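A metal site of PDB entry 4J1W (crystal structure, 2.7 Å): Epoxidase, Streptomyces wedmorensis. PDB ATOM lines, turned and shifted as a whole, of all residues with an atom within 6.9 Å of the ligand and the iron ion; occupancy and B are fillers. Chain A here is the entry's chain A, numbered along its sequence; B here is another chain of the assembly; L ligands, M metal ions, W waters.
O4 of the ligand lies within salt-bridge range of NH2 of Arg 97, at 2.6 Å.
OH of Tyr 105 sits at hydrogen-bond distance from O2 of the ligand.
The side-chain amide nitrogen (ND2) of Asn 135 is in hydrogen-bond range of an oxygen (O4) of the ligand, 2.9 Å away.
An oxygen (O2) of the ligand is in salt-bridge range of the side-chain amino group (NZ) of Lys 23 of chain B (3.0 Å).
O of Glu 142 lies within hydrogen-bond range of N of Val 174, at 3.0 Å.
The backbone NH of His 180 is in hydrogen-bond range of the side-chain amide oxygen of Asn 135 (3.2 Å).
A ring nitrogen (ND1) of His 180 sits at hydrogen-bond distance from the backbone carbonyl oxygen (O) of Val 178, at 2.6 Å.
The guanidinium group (NH1) of Arg 97 lies within hydrogen-bond range of the backbone carbonyl oxygen (O) of Lys 133 (2.7 Å).
OD1 of Asn 135 lies within hydrogen-bond range of N of Gly 137 (2.7 Å).
N of Phe 182 lies within hydrogen-bond range of OH of Tyr 103 (3.0 Å).
The backbone carbonyl oxygen (O) of Leu 193 lies within hydrogen-bond range of the backbone NH (N) of Val 122, at 2.7 Å.
CE1 of Phe 182 touches C3 of the ligand (3.7 Å).
CD1 of Leu 193 touches C3 of the ligand (3.9 Å).
Hydrophobic or aromatic side chains within 4 Å of the ligand: Tyr 105, His 138, His 180, Phe 182 and Leu 193.
Of the 25 residues printed, 9 come within 4 Å of the ligand.
Along chain A the residues within 4 Å of the ligand span positions 97 to 193.
Asn 135 touches the iron ion.
The nearest printed residue that does not touch the iron ion is Asn 197 (4.3 Å).
The iron ion is bound by an oxygen (O3) of the ligand (2.1 Å), an oxygen (O1) of the ligand (2.1 Å), a ring nitrogen (NE2) of His 138 (2.2 Å), the side-chain carboxylate (OE1) of Glu 142 (2.2 Å) and a ring nitrogen (NE2) of His 180 (2.3 Å).
The iron ion has five donor atoms within binding distance.
Water W2 bridges ND2 of Asn 197 (3.0 Å) and OE2 of Glu 142 (3.0 Å).
Water W1 lies within hydrogen-bond range of the backbone carbonyl oxygen of His 180, the side-chain hydroxyl of Tyr 103, the guanidinium group of Arg 97, an oxygen (O4) of the ligand and the side-chain amide nitrogen of Asn 135.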
ATOM      1  N   ARG A  97      17.003 -20.001  13.014  1.00  0.00           N
ATOM      2  CA  ARG A  97      16.471 -20.382  14.315  1.00  0.00           C
ATOM      3  C   ARG A  97      15.440 -19.334  14.725  1.00  0.00           C
ATOM      4  O   ARG A  97      15.795 -18.164  14.954  1.00  0.00           O
ATOM      5  CB  ARG A  97      17.587 -20.461  15.363  1.00  0.00           C
ATOM      6  CG  ARG A  97      18.671 -21.464  14.995  1.00  0.00           C
ATOM      7  CD  ARG A  97      19.608 -21.759  16.149  1.00  0.00           C
ATOM      8  NE  ARG A  97      20.644 -22.696  15.729  1.00  0.00           N
ATOM      9  CZ  ARG A  97      21.566 -23.220  16.531  1.00  0.00           C
ATOM     10  NH1 ARG A  97      21.605 -22.908  17.816  1.00  0.00           N
ATOM     11  NH2 ARG A  97      22.460 -24.062  16.028  1.00  0.00           N
ATOM     12  N   TYR A 103      22.903 -18.125  11.824  1.00  0.00           N
ATOM     13  CA  TYR A 103      24.236 -18.469  11.365  1.00  0.00           C
ATOM     14  C   TYR A 103      24.296 -18.556   9.845  1.00  0.00           C
ATOM     15  O   TYR A 103      23.270 -18.505   9.170  1.00  0.00           O
ATOM     16  CB  TYR A 103      24.647 -19.828  11.923  1.00  0.00           C
ATOM     17  CG  TYR A 103      24.773 -19.944  13.423  1.00  0.00           C
ATOM     18  CD1 TYR A 103      24.537 -21.178  14.068  1.00  0.00           C
ATOM     19  CD2 TYR A 103      25.197 -18.864  14.209  1.00  0.00           C
ATOM     20  CE1 TYR A 103      24.719 -21.328  15.435  1.00  0.00           C
ATOM     21  CE2 TYR A 103      25.378 -19.009  15.595  1.00  0.00           C
ATOM     22  CZ  TYR A 103      25.133 -20.253  16.201  1.00  0.00           C
ATOM     23  OH  TYR A 103      25.304 -20.414  17.560  1.00  0.00           O
ATOM     24  N   TYR A 105      26.600 -21.069   7.436  1.00  0.00           N
ATOM     25  CA  TYR A 105      27.613 -22.115   7.409  1.00  0.00           C
ATOM     26  C   TYR A 105      28.388 -22.252   6.115  1.00  0.00           C
ATOM     27  O   TYR A 105      27.816 -22.562   5.069  1.00  0.00           O
ATOM     28  CB  TYR A 105      26.989 -23.470   7.731  1.00  0.00           C
ATOM     29  CG  TYR A 105      26.265 -23.548   9.035  1.00  0.00           C
ATOM     30  CD1 TYR A 105      24.898 -23.280   9.119  1.00  0.00           C
ATOM     31  CD2 TYR A 105      26.927 -23.922  10.201  1.00  0.00           C
ATOM     32  CE1 TYR A 105      24.217 -23.407  10.303  1.00  0.00           C
ATOM     33  CE2 TYR A 105      26.253 -24.058  11.398  1.00  0.00           C
ATOM     34  CZ  TYR A 105      24.898 -23.802  11.444  1.00  0.00           C
ATOM     35  OH  TYR A 105      24.209 -23.979  12.631  1.00  0.00           O
ATOM     36  N   LEU A 120      33.662 -26.179   9.791  1.00  0.00           N
ATOM     37  CA  LEU A 120      32.892 -25.073   9.249  1.00  0.00           C
ATOM     38  C   LEU A 120      33.419 -23.688   9.601  1.00  0.00           C
ATOM     39  O   LEU A 120      34.037 -23.490  10.648  1.00  0.00           O
ATOM     40  CB  LEU A 120      31.466 -25.144   9.789  1.00  0.00           C
ATOM     41  CG  LEU A 120      30.733 -26.474   9.715  1.00  0.00           C
ATOM     42  CD1 LEU A 120      29.701 -26.535  10.827  1.00  0.00           C
ATOM     43  CD2 LEU A 120      30.066 -26.617   8.340  1.00  0.00           C
ATOM     44  N   VAL A 122      31.821 -20.337  10.443  1.00  0.00           N
ATOM     45  CA  VAL A 122      30.465 -19.891  10.727  1.00  0.00           C
ATOM     46  C   VAL A 122      30.321 -18.388  10.929  1.00  0.00           C
ATOM     47  O   VAL A 122      30.964 -17.800  11.807  1.00  0.00           O
ATOM     48  CB  VAL A 122      29.922 -20.582  12.000  1.00  0.00           C
ATOM     49  CG1 VAL A 122      28.506 -20.127  12.279  1.00  0.00           C
ATOM     50  CG2 VAL A 122      29.991 -22.098  11.820  1.00  0.00           C
ATOM     51  N   VAL A 124      28.448 -15.525  12.404  1.00  0.00           N
ATOM     52  CA  VAL A 124      27.485 -15.324  13.477  1.00  0.00           C
ATOM     53  C   VAL A 124      26.831 -13.968  13.192  1.00  0.00           C
ATOM     54  O   VAL A 124      27.435 -12.917  13.400  1.00  0.00           O
ATOM     55  CB  VAL A 124      28.185 -15.316  14.839  1.00  0.00           C
ATOM     56  CG1 VAL A 124      27.159 -15.189  15.951  1.00  0.00           C
ATOM     57  CG2 VAL A 124      28.991 -16.580  15.011  1.00  0.00           C
ATOM     58  N   LYS A 133      19.947 -18.370  20.570  1.00  0.00           N
ATOM     59  CA  LYS A 133      19.142 -19.545  20.253  1.00  0.00           C
ATOM     60  C   LYS A 133      19.966 -20.822  20.429  1.00  0.00           C
ATOM     61  O   LYS A 133      20.909 -21.068  19.680  1.00  0.00           O
ATOM     62  CB  LYS A 133      18.627 -19.424  18.820  1.00  0.00           C
ATOM     63  CG  LYS A 133      17.738 -18.206  18.586  1.00  0.00           C
ATOM     64  CD  LYS A 133      16.341 -18.402  19.182  1.00  0.00           C
ATOM     65  CE  LYS A 133      15.526 -17.114  19.170  1.00  0.00           C
ATOM     66  NZ  LYS A 133      16.021 -16.134  20.172  1.00  0.00           N
ATOM     67  N   PHE A 134      19.602 -21.616  21.425  1.00  0.00           N
ATOM     68  CA  PHE A 134      20.299 -22.867  21.734  1.00  0.00           C
ATOM     69  C   PHE A 134      19.980 -24.053  20.847  1.00  0.00           C
ATOM     70  O   PHE A 134      18.847 -24.218  20.395  1.00  0.00           O
ATOM     71  CB  PHE A 134      19.970 -23.318  23.166  1.00  0.00           C
ATOM     72  CG  PHE A 134      20.817 -22.693  24.218  1.00  0.00           C
ATOM     73  CD1 PHE A 134      20.707 -21.338  24.513  1.00  0.00           C
ATOM     74  CD2 PHE A 134      21.699 -23.468  24.962  1.00  0.00           C
ATOM     75  CE1 PHE A 134      21.458 -20.770  25.535  1.00  0.00           C
ATOM     76  CE2 PHE A 134      22.448 -22.909  25.987  1.00  0.00           C
ATOM     77  CZ  PHE A 134      22.329 -21.555  26.272  1.00  0.00           C
ATOM     78  N   ASN A 135      20.989 -24.875  20.602  1.00  0.00           N
ATOM     79  CA  ASN A 135      20.783 -26.111  19.868  1.00  0.00           C
ATOM     80  C   ASN A 135      20.598 -27.031  21.081  1.00  0.00           C
ATOM     81  O   ASN A 135      20.827 -26.592  22.214  1.00  0.00           O
ATOM     82  CB  ASN A 135      22.020 -26.521  19.071  1.00  0.00           C
ATOM     83  CG  ASN A 135      23.265 -26.651  19.930  1.00  0.00           C
ATOM     84  OD1 ASN A 135      23.214 -27.155  21.054  1.00  0.00           O
ATOM     85  ND2 ASN A 135      24.396 -26.219  19.394  1.00  0.00           N
ATOM     86  N   SER A 136      20.200 -28.270  20.881  1.00  0.00           N
ATOM     87  CA  SER A 136      19.984 -29.166  22.014  1.00  0.00           C
ATOM     88  C   SER A 136      21.188 -30.069  22.276  1.00  0.00           C
ATOM     89  O   SER A 136      21.029 -31.171  22.794  1.00  0.00           O
ATOM     90  CB  SER A 136      18.741 -30.019  21.780  1.00  0.00           C
ATOM     91  OG  SER A 136      18.840 -30.706  20.541  1.00  0.00           O
ATOM     92  N   GLY A 137      22.379 -29.605  21.931  1.00  0.00           N
ATOM     93  CA  GLY A 137      23.560 -30.421  22.117  1.00  0.00           C
ATOM     94  C   GLY A 137      23.574 -31.439  20.998  1.00  0.00           C
ATOM     95  O   GLY A 137      22.518 -31.771  20.439  1.00  0.00           O
ATOM     96  N   HIS A 138      24.747 -31.943  20.629  1.00  0.00           N
ATOM     97  CA  HIS A 138      24.834 -32.917  19.563  1.00  0.00           C
ATOM     98  C   HIS A 138      25.958 -33.921  19.757  1.00  0.00           C
ATOM     99  O   HIS A 138      26.870 -33.702  20.549  1.00  0.00           O
ATOM    100  CB  HIS A 138      24.991 -32.211  18.199  1.00  0.00           C
ATOM    101  CG  HIS A 138      26.112 -31.213  18.161  1.00  0.00           C
ATOM    102  ND1 HIS A 138      27.445 -31.534  18.287  1.00  0.00           N
ATOM    103  CD2 HIS A 138      26.084 -29.868  18.005  1.00  0.00           C
ATOM    104  CE1 HIS A 138      28.161 -30.410  18.209  1.00  0.00           C
ATOM    105  NE2 HIS A 138      27.365 -29.368  18.037  1.00  0.00           N
ATOM    106  N   GLU A 142      33.350 -30.858  19.746  1.00  0.00           N
ATOM    107  CA  GLU A 142      33.518 -29.767  18.806  1.00  0.00           C
ATOM    108  C   GLU A 142      34.588 -28.795  19.260  1.00  0.00           C
ATOM    109  O   GLU A 142      34.645 -28.412  20.433  1.00  0.00           O
ATOM    110  CB  GLU A 142      32.183 -29.043  18.619  1.00  0.00           C
ATOM    111  CG  GLU A 142      32.236 -27.739  17.855  1.00  0.00           C
ATOM    112  CD  GLU A 142      30.845 -27.192  17.560  1.00  0.00           C
ATOM    113  OE1 GLU A 142      29.894 -27.538  18.286  1.00  0.00           O
ATOM    114  OE2 GLU A 142      30.709 -26.405  16.600  1.00  0.00           O
ATOM    115  N   LEU A 144      36.280 -25.045  18.646  1.00  0.00           N
ATOM    116  CA  LEU A 144      35.953 -23.724  18.113  1.00  0.00           C
ATOM    117  C   LEU A 144      37.147 -22.785  18.207  1.00  0.00           C
ATOM    118  O   LEU A 144      37.985 -22.920  19.084  1.00  0.00           O
ATOM    119  CB  LEU A 144      34.798 -23.088  18.902  1.00  0.00           C
ATOM    120  CG  LEU A 144      33.365 -23.627  18.948  1.00  0.00           C
ATOM    121  CD1 LEU A 144      32.740 -23.535  17.571  1.00  0.00           C
ATOM    122  CD2 LEU A 144      33.344 -25.057  19.457  1.00  0.00           C
ATOM    123  N   VAL A 174      33.804 -28.079  23.260  1.00  0.00           N
ATOM    124  CA  VAL A 174      32.490 -28.384  23.774  1.00  0.00           C
ATOM    125  C   VAL A 174      32.285 -29.876  23.640  1.00  0.00           C
ATOM    126  O   VAL A 174      32.257 -30.396  22.517  1.00  0.00           O
ATOM    127  CB  VAL A 174      31.383 -27.650  22.981  1.00  0.00           C
ATOM    128  CG1 VAL A 174      30.003 -28.073  23.484  1.00  0.00           C
ATOM    129  CG2 VAL A 174      31.560 -26.147  23.100  1.00  0.00           C
ATOM    130  N   VAL A 178      26.504 -31.411  24.958  1.00  0.00           N
ATOM    131  CA  VAL A 178      26.428 -30.196  25.761  1.00  0.00           C
ATOM    132  C   VAL A 178      25.736 -29.142  24.883  1.00  0.00           C
ATOM    133  O   VAL A 178      26.238 -28.784  23.826  1.00  0.00           O
ATOM    134  CB  VAL A 178      27.819 -29.659  26.150  1.00  0.00           C
ATOM    135  CG1 VAL A 178      27.684 -28.365  26.939  1.00  0.00           C
ATOM    136  CG2 VAL A 178      28.579 -30.704  26.944  1.00  0.00           C
ATOM    137  N   HIS A 180      24.712 -25.644  23.431  1.00  0.00           N
ATOM    138  CA  HIS A 180      25.438 -24.375  23.355  1.00  0.00           C
ATOM    139  C   HIS A 180      24.772 -23.399  22.396  1.00  0.00           C
ATOM    140  O   HIS A 180      23.929 -23.777  21.598  1.00  0.00           O
ATOM    141  CB  HIS A 180      26.893 -24.627  22.916  1.00  0.00           C
ATOM    142  CG  HIS A 180      27.027 -25.647  21.823  1.00  0.00           C
ATOM    143  ND1 HIS A 180      26.838 -27.001  22.014  1.00  0.00           N
ATOM    144  CD2 HIS A 180      27.296 -25.502  20.505  1.00  0.00           C
ATOM    145  CE1 HIS A 180      26.981 -27.627  20.833  1.00  0.00           C
ATOM    146  NE2 HIS A 180      27.261 -26.755  19.885  1.00  0.00           N
ATOM    147  N   ALA A 181      25.182 -22.129  22.484  1.00  0.00           N
ATOM    148  CA  ALA A 181      24.648 -21.096  21.618  1.00  0.00           C
ATOM    149  C   ALA A 181      25.634 -19.939  21.510  1.00  0.00           C
ATOM    150  O   ALA A 181      26.350 -19.650  22.484  1.00  0.00           O
ATOM    151  CB  ALA A 181      23.322 -20.583  22.166  1.00  0.00           C
ATOM    152  N   PHE A 182      25.676 -19.297  20.347  1.00  0.00           N
ATOM    153  CA  PHE A 182      26.585 -18.165  20.139  1.00  0.00           C
ATOM    154  C   PHE A 182      25.895 -16.982  19.465  1.00  0.00           C
ATOM    155  O   PHE A 182      24.925 -17.143  18.737  1.00  0.00           O
ATOM    156  CB  PHE A 182      27.754 -18.546  19.217  1.00  0.00           C
ATOM    157  CG  PHE A 182      28.487 -19.778  19.616  1.00  0.00           C
ATOM    158  CD1 PHE A 182      28.125 -21.018  19.085  1.00  0.00           C
ATOM    159  CD2 PHE A 182      29.543 -19.707  20.528  1.00  0.00           C
ATOM    160  CE1 PHE A 182      28.820 -22.168  19.460  1.00  0.00           C
ATOM    161  CE2 PHE A 182      30.250 -20.846  20.910  1.00  0.00           C
ATOM    162  CZ  PHE A 182      29.877 -22.084  20.378  1.00  0.00           C
ATOM    163  N   LEU A 193      33.528 -17.508  13.396  1.00  0.00           N
ATOM    164  CA  LEU A 193      34.367 -18.504  14.035  1.00  0.00           C
ATOM    165  C   LEU A 193      34.515 -19.785  13.222  1.00  0.00           C
ATOM    166  O   LEU A 193      33.771 -20.025  12.296  1.00  0.00           O
ATOM    167  CB  LEU A 193      33.816 -18.815  15.430  1.00  0.00           C
ATOM    168  CG  LEU A 193      32.407 -19.358  15.550  1.00  0.00           C
ATOM    169  CD1 LEU A 193      32.408 -20.796  15.077  1.00  0.00           C
ATOM    170  CD2 LEU A 193      31.937 -19.279  16.996  1.00  0.00           C
ATOM    171  N   ILE A 194      35.525 -20.572  13.569  1.00  0.00           N
ATOM    172  CA  ILE A 194      35.774 -21.853  12.895  1.00  0.00           C
ATOM    173  C   ILE A 194      35.286 -22.910  13.855  1.00  0.00           C
ATOM    174  O   ILE A 194      35.623 -22.916  15.032  1.00  0.00           O
ATOM    175  CB  ILE A 194      37.280 -22.087  12.630  1.00  0.00           C
ATOM    176  CG1 ILE A 194      37.801 -21.033  11.640  1.00  0.00           C
ATOM    177  CG2 ILE A 194      37.488 -23.471  12.055  1.00  0.00           C
ATOM    178  CD1 ILE A 194      39.219 -21.259  11.203  1.00  0.00           C
ATOM    179  N   ALA A 195      34.452 -23.807  13.347  1.00  0.00           N
ATOM    180  CA  ALA A 195      33.911 -24.869  14.182  1.00  0.00           C
ATOM    181  C   ALA A 195      34.281 -26.195  13.566  1.00  0.00           C
ATOM    182  O   ALA A 195      33.955 -26.466  12.415  1.00  0.00           O
ATOM    183  CB  ALA A 195      32.405 -24.733  14.277  1.00  0.00           C
ATOM    184  N   ASN A 197      33.776 -30.139  14.069  1.00  0.00           N
ATOM    185  CA  ASN A 197      33.127 -31.269  14.743  1.00  0.00           C
ATOM    186  C   ASN A 197      33.902 -32.488  14.330  1.00  0.00           C
ATOM    187  O   ASN A 197      34.207 -32.666  13.155  1.00  0.00           O
ATOM    188  CB  ASN A 197      31.676 -31.395  14.290  1.00  0.00           C
ATOM    189  CG  ASN A 197      30.881 -30.131  14.513  1.00  0.00           C
ATOM    190  OD1 ASN A 197      30.367 -29.889  15.611  1.00  0.00           O
ATOM    191  ND2 ASN A 197      30.798 -29.301  13.470  1.00  0.00           N
ATOM    192  N   GLU B  20      21.612 -33.045   8.964  1.00  0.00           N
ATOM    193  CA  GLU B  20      21.817 -31.902   9.818  1.00  0.00           C
ATOM    194  C   GLU B  20      23.274 -31.688  10.216  1.00  0.00           C
ATOM    195  O   GLU B  20      23.725 -30.558  10.314  1.00  0.00           O
ATOM    196  CB  GLU B  20      20.968 -32.022  11.087  1.00  0.00           C
ATOM    197  CG  GLU B  20      19.483 -31.928  10.810  1.00  0.00           C
ATOM    198  CD  GLU B  20      18.635 -31.977  12.071  1.00  0.00           C
ATOM    199  OE1 GLU B  20      17.405 -31.770  11.969  1.00  0.00           O
ATOM    200  OE2 GLU B  20      19.197 -32.228  13.168  1.00  0.00           O
ATOM    201  N   LYS B  23      25.115 -29.845   7.602  1.00  0.00           N
ATOM    202  CA  LYS B  23      24.402 -28.605   7.357  1.00  0.00           C
ATOM    203  C   LYS B  23      23.497 -28.480   6.138  1.00  0.00           C
ATOM    204  O   LYS B  23      23.131 -27.361   5.763  1.00  0.00           O
ATOM    205  CB  LYS B  23      25.400 -27.455   7.345  1.00  0.00           C
ATOM    206  CG  LYS B  23      26.276 -27.414   8.580  1.00  0.00           C
ATOM    207  CD  LYS B  23      25.436 -27.474   9.843  1.00  0.00           C
ATOM    208  CE  LYS B  23      26.331 -27.598  11.062  1.00  0.00           C
ATOM    209  NZ  LYS B  23      25.569 -27.757  12.314  1.00  0.00           N
HETATM  210  C1  LIG L   1      28.005 -23.714  15.300  1.00  0.00           C
HETATM  211  O1  LIG L   1      28.266 -25.254  17.149  1.00  0.00           O
HETATM  212  P1  LIG L   1      25.981 -25.671  15.801  1.00  0.00           P
HETATM  213  C2  LIG L   1      27.319 -24.510  16.410  1.00  0.00           C
HETATM  214  O2  LIG L   1      25.750 -25.489  14.330  1.00  0.00           O
HETATM  215  C3  LIG L   1      29.089 -22.757  15.822  1.00  0.00           C
HETATM  216  O3  LIG L   1      26.416 -27.210  16.097  1.00  0.00           O
HETATM  217  O4  LIG L   1      24.646 -25.365  16.623  1.00  0.00           O
HETATM  218 FE    FE M   1      27.769 -27.240  17.733  1.00  0.00          FE
HETATM  219  O   HOH W   1      24.441 -23.002  18.837  1.00  0.00           O
HETATM  220  O   HOH W   2      28.910 -27.184  14.311  1.00  0.00           O
